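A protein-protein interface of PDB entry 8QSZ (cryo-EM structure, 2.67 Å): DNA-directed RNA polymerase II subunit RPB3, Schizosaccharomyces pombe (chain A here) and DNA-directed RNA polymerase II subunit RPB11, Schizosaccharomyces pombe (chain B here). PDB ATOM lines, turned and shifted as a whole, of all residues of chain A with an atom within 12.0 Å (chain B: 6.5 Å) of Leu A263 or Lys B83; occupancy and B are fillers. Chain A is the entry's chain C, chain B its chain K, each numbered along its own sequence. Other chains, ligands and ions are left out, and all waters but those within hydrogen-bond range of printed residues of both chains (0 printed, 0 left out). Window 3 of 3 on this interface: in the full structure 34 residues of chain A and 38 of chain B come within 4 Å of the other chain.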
ATOM      1  N   GLU A 254     -10.813 -16.461 -24.114  1.00  0.00           N
ATOM      2  CA  GLU A 254     -11.239 -16.148 -25.471  1.00  0.00           C
ATOM      3  C   GLU A 254     -11.198 -17.374 -26.375  1.00  0.00           C
ATOM      4  O   GLU A 254     -12.038 -17.504 -27.271  1.00  0.00           O
ATOM      5  CB  GLU A 254     -10.373 -15.030 -26.045  1.00  0.00           C
ATOM      6  CG  GLU A 254     -10.761 -14.606 -27.448  1.00  0.00           C
ATOM      7  CD  GLU A 254     -12.216 -14.199 -27.557  1.00  0.00           C
ATOM      8  OE1 GLU A 254     -12.811 -13.811 -26.530  1.00  0.00           O
ATOM      9  OE2 GLU A 254     -12.767 -14.267 -28.675  1.00  0.00           O
ATOM     10  N   LYS A 255     -10.245 -18.282 -26.166  1.00  0.00           N
ATOM     11  CA  LYS A 255     -10.267 -19.541 -26.907  1.00  0.00           C
ATOM     12  C   LYS A 255     -11.540 -20.320 -26.604  1.00  0.00           C
ATOM     13  O   LYS A 255     -12.233 -20.798 -27.515  1.00  0.00           O
ATOM     14  CB  LYS A 255      -9.036 -20.379 -26.563  1.00  0.00           C
ATOM     15  CG  LYS A 255      -7.719 -19.670 -26.782  1.00  0.00           C
ATOM     16  CD  LYS A 255      -6.660 -20.606 -27.328  1.00  0.00           C
ATOM     17  CE  LYS A 255      -6.167 -21.557 -26.260  1.00  0.00           C
ATOM     18  NZ  LYS A 255      -5.196 -20.907 -25.353  1.00  0.00           N
ATOM     19  N   LEU A 256     -11.878 -20.437 -25.318  1.00  0.00           N
ATOM     20  CA  LEU A 256     -13.102 -21.142 -24.949  1.00  0.00           C
ATOM     21  C   LEU A 256     -14.331 -20.440 -25.513  1.00  0.00           C
ATOM     22  O   LEU A 256     -15.290 -21.094 -25.938  1.00  0.00           O
ATOM     23  CB  LEU A 256     -13.203 -21.255 -23.432  1.00  0.00           C
ATOM     24  CG  LEU A 256     -12.205 -22.196 -22.766  1.00  0.00           C
ATOM     25  CD1 LEU A 256     -11.972 -21.780 -21.330  1.00  0.00           C
ATOM     26  CD2 LEU A 256     -12.687 -23.629 -22.841  1.00  0.00           C
ATOM     27  N   ALA A 257     -14.328 -19.108 -25.510  1.00  0.00           N
ATOM     28  CA  ALA A 257     -15.472 -18.354 -26.009  1.00  0.00           C
ATOM     29  C   ALA A 257     -15.641 -18.529 -27.510  1.00  0.00           C
ATOM     30  O   ALA A 257     -16.769 -18.614 -28.003  1.00  0.00           O
ATOM     31  CB  ALA A 257     -15.315 -16.879 -25.656  1.00  0.00           C
ATOM     32  N   VAL A 258     -14.538 -18.567 -28.256  1.00  0.00           N
ATOM     33  CA  VAL A 258     -14.628 -18.865 -29.682  1.00  0.00           C
ATOM     34  C   VAL A 258     -15.216 -20.252 -29.886  1.00  0.00           C
ATOM     35  O   VAL A 258     -16.071 -20.460 -30.756  1.00  0.00           O
ATOM     36  CB  VAL A 258     -13.248 -18.733 -30.351  1.00  0.00           C
ATOM     37  CG1 VAL A 258     -13.250 -19.403 -31.716  1.00  0.00           C
ATOM     38  CG2 VAL A 258     -12.862 -17.272 -30.477  1.00  0.00           C
ATOM     39  N   LEU A 259     -14.767 -21.222 -29.090  1.00  0.00           N
ATOM     40  CA  LEU A 259     -15.342 -22.562 -29.180  1.00  0.00           C
ATOM     41  C   LEU A 259     -16.851 -22.520 -28.966  1.00  0.00           C
ATOM     42  O   LEU A 259     -17.620 -23.087 -29.751  1.00  0.00           O
ATOM     43  CB  LEU A 259     -14.673 -23.477 -28.154  1.00  0.00           C
ATOM     44  CG  LEU A 259     -15.242 -24.884 -27.990  1.00  0.00           C
ATOM     45  CD1 LEU A 259     -15.073 -25.691 -29.262  1.00  0.00           C
ATOM     46  CD2 LEU A 259     -14.567 -25.567 -26.820  1.00  0.00           C
ATOM     47  N   VAL A 260     -17.290 -21.836 -27.910  1.00  0.00           N
ATOM     48  CA  VAL A 260     -18.715 -21.774 -27.590  1.00  0.00           C
ATOM     49  C   VAL A 260     -19.488 -21.116 -28.724  1.00  0.00           C
ATOM     50  O   VAL A 260     -20.532 -21.614 -29.158  1.00  0.00           O
ATOM     51  CB  VAL A 260     -18.936 -21.028 -26.264  1.00  0.00           C
ATOM     52  CG1 VAL A 260     -20.409 -20.728 -26.070  1.00  0.00           C
ATOM     53  CG2 VAL A 260     -18.404 -21.838 -25.113  1.00  0.00           C
ATOM     54  N   ARG A 261     -18.989 -19.984 -29.219  1.00  0.00           N
ATOM     55  CA  ARG A 261     -19.688 -19.274 -30.284  1.00  0.00           C
ATOM     56  C   ARG A 261     -19.811 -20.137 -31.529  1.00  0.00           C
ATOM     57  O   ARG A 261     -20.856 -20.143 -32.189  1.00  0.00           O
ATOM     58  CB  ARG A 261     -18.959 -17.974 -30.616  1.00  0.00           C
ATOM     59  CG  ARG A 261     -19.099 -16.891 -29.565  1.00  0.00           C
ATOM     60  CD  ARG A 261     -18.664 -15.535 -30.107  1.00  0.00           C
ATOM     61  NE  ARG A 261     -17.213 -15.404 -30.161  1.00  0.00           N
ATOM     62  CZ  ARG A 261     -16.467 -14.847 -29.216  1.00  0.00           C
ATOM     63  NH1 ARG A 261     -16.999 -14.350 -28.112  1.00  0.00           N
ATOM     64  NH2 ARG A 261     -15.149 -14.786 -29.384  1.00  0.00           N
ATOM     65  N   ASP A 262     -18.750 -20.866 -31.876  1.00  0.00           N
ATOM     66  CA  ASP A 262     -18.788 -21.673 -33.088  1.00  0.00           C
ATOM     67  C   ASP A 262     -19.724 -22.865 -32.932  1.00  0.00           C
ATOM     68  O   ASP A 262     -20.430 -23.230 -33.877  1.00  0.00           O
ATOM     69  CB  ASP A 262     -17.378 -22.130 -33.449  1.00  0.00           C
ATOM     70  CG  ASP A 262     -16.494 -20.982 -33.903  1.00  0.00           C
ATOM     71  OD1 ASP A 262     -17.027 -20.002 -34.461  1.00  0.00           O
ATOM     72  OD2 ASP A 262     -15.267 -21.052 -33.690  1.00  0.00           O
ATOM     73  N   LEU A 263     -19.740 -23.493 -31.754  1.00  0.00           N
ATOM     74  CA  LEU A 263     -20.631 -24.634 -31.555  1.00  0.00           C
ATOM     75  C   LEU A 263     -22.083 -24.187 -31.440  1.00  0.00           C
ATOM     76  O   LEU A 263     -22.972 -24.768 -32.071  1.00  0.00           O
ATOM     77  CB  LEU A 263     -20.214 -25.426 -30.317  1.00  0.00           C
ATOM     78  CG  LEU A 263     -19.040 -26.387 -30.500  1.00  0.00           C
ATOM     79  CD1 LEU A 263     -18.713 -27.050 -29.182  1.00  0.00           C
ATOM     80  CD2 LEU A 263     -19.334 -27.432 -31.560  1.00  0.00           C
ATOM     81  N   ASP A 264     -22.344 -23.159 -30.641  1.00  0.00           N
ATOM     82  CA  ASP A 264     -23.698 -22.634 -30.504  1.00  0.00           C
ATOM     83  C   ASP A 264     -24.169 -22.062 -31.838  1.00  0.00           C
ATOM     84  O   ASP A 264     -25.132 -21.299 -31.896  1.00  0.00           O
ATOM     85  CB  ASP A 264     -23.760 -21.561 -29.415  1.00  0.00           C
ATOM     86  CG  ASP A 264     -24.130 -22.125 -28.058  1.00  0.00           C
ATOM     87  OD1 ASP A 264     -25.028 -22.988 -27.994  1.00  0.00           O
ATOM     88  OD2 ASP A 264     -23.527 -21.701 -27.051  1.00  0.00           O
ATOM     89  N   VAL B  18     -13.868 -24.738 -35.965  1.00  0.00           N
ATOM     90  CA  VAL B  18     -14.496 -25.854 -35.268  1.00  0.00           C
ATOM     91  C   VAL B  18     -15.258 -26.681 -36.290  1.00  0.00           C
ATOM     92  O   VAL B  18     -15.991 -26.131 -37.118  1.00  0.00           O
ATOM     93  CB  VAL B  18     -15.441 -25.371 -34.153  1.00  0.00           C
ATOM     94  CG1 VAL B  18     -15.865 -26.535 -33.279  1.00  0.00           C
ATOM     95  CG2 VAL B  18     -14.779 -24.287 -33.325  1.00  0.00           C
ATOM     96  N   THR B  19     -15.070 -27.995 -36.241  1.00  0.00           N
ATOM     97  CA  THR B  19     -15.858 -28.939 -37.016  1.00  0.00           C
ATOM     98  C   THR B  19     -16.507 -29.909 -36.045  1.00  0.00           C
ATOM     99  O   THR B  19     -15.844 -30.411 -35.137  1.00  0.00           O
ATOM    100  CB  THR B  19     -14.998 -29.696 -38.029  1.00  0.00           C
ATOM    101  OG1 THR B  19     -14.478 -28.777 -38.996  1.00  0.00           O
ATOM    102  CG2 THR B  19     -15.812 -30.756 -38.735  1.00  0.00           C
ATOM    103  N   TYR B  20     -17.798 -30.158 -36.223  1.00  0.00           N
ATOM    104  CA  TYR B  20     -18.555 -31.030 -35.337  1.00  0.00           C
ATOM    105  C   TYR B  20     -19.231 -32.091 -36.186  1.00  0.00           C
ATOM    106  O   TYR B  20     -19.950 -31.761 -37.132  1.00  0.00           O
ATOM    107  CB  TYR B  20     -19.581 -30.224 -34.539  1.00  0.00           C
ATOM    108  CG  TYR B  20     -20.470 -31.036 -33.631  1.00  0.00           C
ATOM    109  CD1 TYR B  20     -21.586 -31.691 -34.125  1.00  0.00           C
ATOM    110  CD2 TYR B  20     -20.206 -31.129 -32.274  1.00  0.00           C
ATOM    111  CE1 TYR B  20     -22.404 -32.422 -33.299  1.00  0.00           C
ATOM    112  CE2 TYR B  20     -21.020 -31.856 -31.441  1.00  0.00           C
ATOM    113  CZ  TYR B  20     -22.117 -32.499 -31.958  1.00  0.00           C
ATOM    114  OH  TYR B  20     -22.933 -33.227 -31.130  1.00  0.00           O
ATOM    115  N   ALA B  30     -19.914 -37.788 -30.504  1.00  0.00           N
ATOM    116  CA  ALA B  30     -19.543 -36.796 -31.495  1.00  0.00           C
ATOM    117  C   ALA B  30     -18.038 -36.590 -31.468  1.00  0.00           C
ATOM    118  O   ALA B  30     -17.376 -36.809 -30.448  1.00  0.00           O
ATOM    119  CB  ALA B  30     -20.257 -35.463 -31.256  1.00  0.00           C
ATOM    120  N   VAL B  32     -15.261 -33.595 -32.398  1.00  0.00           N
ATOM    121  CA  VAL B  32     -15.062 -32.172 -32.613  1.00  0.00           C
ATOM    122  C   VAL B  32     -13.602 -31.972 -32.985  1.00  0.00           C
ATOM    123  O   VAL B  32     -12.708 -32.263 -32.184  1.00  0.00           O
ATOM    124  CB  VAL B  32     -15.428 -31.353 -31.365  1.00  0.00           C
ATOM    125  CG1 VAL B  32     -15.337 -29.870 -31.656  1.00  0.00           C
ATOM    126  CG2 VAL B  32     -16.811 -31.721 -30.883  1.00  0.00           C
ATOM    127  N   THR B  76     -22.163 -38.867 -24.523  1.00  0.00           N
ATOM    128  CA  THR B  76     -23.005 -38.505 -23.395  1.00  0.00           C
ATOM    129  C   THR B  76     -24.105 -39.540 -23.202  1.00  0.00           C
ATOM    130  O   THR B  76     -24.290 -40.451 -24.009  1.00  0.00           O
ATOM    131  CB  THR B  76     -23.634 -37.125 -23.599  1.00  0.00           C
ATOM    132  OG1 THR B  76     -24.473 -37.150 -24.754  1.00  0.00           O
ATOM    133  CG2 THR B  76     -22.568 -36.080 -23.789  1.00  0.00           C
ATOM    134  N   SER B  81     -26.866 -34.191 -25.257  1.00  0.00           N
ATOM    135  CA  SER B  81     -26.115 -34.182 -26.502  1.00  0.00           C
ATOM    136  C   SER B  81     -24.650 -33.841 -26.243  1.00  0.00           C
ATOM    137  O   SER B  81     -24.337 -33.121 -25.292  1.00  0.00           O
ATOM    138  CB  SER B  81     -26.697 -33.164 -27.487  1.00  0.00           C
ATOM    139  OG  SER B  81     -26.035 -33.227 -28.736  1.00  0.00           O
ATOM    140  N   PRO B  82     -23.723 -34.347 -27.063  1.00  0.00           N
ATOM    141  CA  PRO B  82     -22.314 -33.958 -26.877  1.00  0.00           C
ATOM    142  C   PRO B  82     -22.087 -32.464 -27.005  1.00  0.00           C
ATOM    143  O   PRO B  82     -21.268 -31.893 -26.275  1.00  0.00           O
ATOM    144  CB  PRO B  82     -21.586 -34.740 -27.981  1.00  0.00           C
ATOM    145  CG  PRO B  82     -22.510 -35.826 -28.365  1.00  0.00           C
ATOM    146  CD  PRO B  82     -23.886 -35.293 -28.178  1.00  0.00           C
ATOM    147  N   LYS B  83     -22.805 -31.811 -27.920  1.00  0.00           N
ATOM    148  CA  LYS B  83     -22.612 -30.383 -28.139  1.00  0.00           C
ATOM    149  C   LYS B  83     -22.985 -29.585 -26.897  1.00  0.00           C
ATOM    150  O   LYS B  83     -22.283 -28.641 -26.516  1.00  0.00           O
ATOM    151  CB  LYS B  83     -23.440 -29.935 -29.343  1.00  0.00           C
ATOM    152  CG  LYS B  83     -23.198 -28.502 -29.767  1.00  0.00           C
ATOM    153  CD  LYS B  83     -24.107 -28.103 -30.914  1.00  0.00           C
ATOM    154  CE  LYS B  83     -23.670 -28.743 -32.219  1.00  0.00           C
ATOM    155  NZ  LYS B  83     -24.472 -28.275 -33.378  1.00  0.00           N
ATOM    156  N   GLN B  84     -24.092 -29.952 -26.251  1.00  0.00           N
ATOM    157  CA  GLN B  84     -24.520 -29.228 -25.060  1.00  0.00           C
ATOM    158  C   GLN B  84     -23.525 -29.385 -23.918  1.00  0.00           C
ATOM    159  O   GLN B  84     -23.219 -28.414 -23.221  1.00  0.00           O
ATOM    160  CB  GLN B  84     -25.909 -29.694 -24.628  1.00  0.00           C
ATOM    161  CG  GLN B  84     -27.026 -29.223 -25.541  1.00  0.00           C
ATOM    162  CD  GLN B  84     -28.256 -30.104 -25.467  1.00  0.00           C
ATOM    163  OE1 GLN B  84     -28.188 -31.308 -25.703  1.00  0.00           O
ATOM    164  NE2 GLN B  84     -29.394 -29.503 -25.141  1.00  0.00           N
ATOM    165  N   VAL B  85     -23.008 -30.597 -23.703  1.00  0.00           N
ATOM    166  CA  VAL B  85     -22.045 -30.783 -22.620  1.00  0.00           C
ATOM    167  C   VAL B  85     -20.752 -30.045 -22.930  1.00  0.00           C
ATOM    168  O   VAL B  85     -20.116 -29.484 -22.032  1.00  0.00           O
ATOM    169  CB  VAL B  85     -21.781 -32.277 -22.352  1.00  0.00           C
ATOM    170  CG1 VAL B  85     -22.968 -32.911 -21.663  1.00  0.00           C
ATOM    171  CG2 VAL B  85     -21.430 -33.009 -23.629  1.00  0.00           C
ATOM    172  N   ILE B  86     -20.331 -30.037 -24.197  1.00  0.00           N
ATOM    173  CA  ILE B  86     -19.120 -29.308 -24.556  1.00  0.00           C
ATOM    174  C   ILE B  86     -19.300 -27.823 -24.281  1.00  0.00           C
ATOM    175  O   ILE B  86     -18.419 -27.171 -23.708  1.00  0.00           O
ATOM    176  CB  ILE B  86     -18.754 -29.565 -26.029  1.00  0.00           C
ATOM    177  CG1 ILE B  86     -18.293 -31.008 -26.219  1.00  0.00           C
ATOM    178  CG2 ILE B  86     -17.668 -28.602 -26.478  1.00  0.00           C
ATOM    179  CD1 ILE B  86     -18.271 -31.453 -27.655  1.00  0.00           C
ATOM    180  N   VAL B  87     -20.444 -27.266 -24.681  1.00  0.00           N
ATOM    181  CA  VAL B  87     -20.694 -25.845 -24.463  1.00  0.00           C
ATOM    182  C   VAL B  87     -20.768 -25.535 -22.973  1.00  0.00           C
ATOM    183  O   VAL B  87     -20.260 -24.506 -22.515  1.00  0.00           O
ATOM    184  CB  VAL B  87     -21.977 -25.414 -25.194  1.00  0.00           C
ATOM    185  CG1 VAL B  87     -22.378 -24.018 -24.774  1.00  0.00           C
ATOM    186  CG2 VAL B  87     -21.774 -25.484 -26.692  1.00  0.00           C
ATOM    187  N   ASP B  88     -21.417 -26.403 -22.196  1.00  0.00           N
ATOM    188  CA  ASP B  88     -21.518 -26.168 -20.760  1.00  0.00           C
ATOM    189  C   ASP B  88     -20.149 -26.213 -20.097  1.00  0.00           C
ATOM    190  O   ASP B  88     -19.848 -25.392 -19.226  1.00  0.00           O
ATOM    191  CB  ASP B  88     -22.451 -27.194 -20.126  1.00  0.00           C
ATOM    192  CG  ASP B  88     -23.878 -27.055 -20.606  1.00  0.00           C
ATOM    193  OD1 ASP B  88     -24.200 -26.031 -21.242  1.00  0.00           O
ATOM    194  OD2 ASP B  88     -24.682 -27.973 -20.345  1.00  0.00           O
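Among the printed residues, merely in contact across the chains: Leu A263 with Ile B86, Asp A262 with Val B18, Asp A264 with Val B87, Leu A263 with Lys B83, Leu A263 with Tyr B20, Leu A263 with Val B87 and Leu A263 with Val B18.
Leu A263 touches just these residues of chain B: Val B18 (3.97 Å), Tyr B20 (3.9 Å), Lys B83 (3.7 Å), Ile B86 (3.3 Å) and Val B87 (3.9 Å). Lys B83 touches just one residue of chain A: Leu A263 (3.7 Å). Of chain A, only Asp A262 and Leu A263 come within 4 Å of Val B18. Tyr B20 touches one residue of chain A. No residue of chain A comes within 4 Å of Ala B30. No residue of chain A comes within 4 Å of Ser B81. No residue of chain A comes within 4 Å of Val B85. Ile B86 touches just one residue of chain A: Leu A263 (3.3 Å). Val B87 touches two residues of chain A. Printed residues of chain B within 4 Å of Asp A264: Val B87 (3.4 Å). Of the printed residues of chain B, Asp A262 touches Val B18. The nearest residue of chain B that does not touch Leu A263 is Val B32 (4.7 Å). The nearest printed residue of chain B that does not touch Asp A264 is Lys B83 (5.3 Å).
Hydrophobic or aromatic side chains of chain A within 4 Å of the printed part of chain B: Leu A263. Hydrophobic or aromatic side chains of chain B within 4 Å of the printed part of chain A: Val B18, Tyr B20, Ile B86 and Val B87. Among the printed residues, no Asp or Glu carboxylate lies within 4 Å of a Lys or Arg side-chain nitrogen of the other chain.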
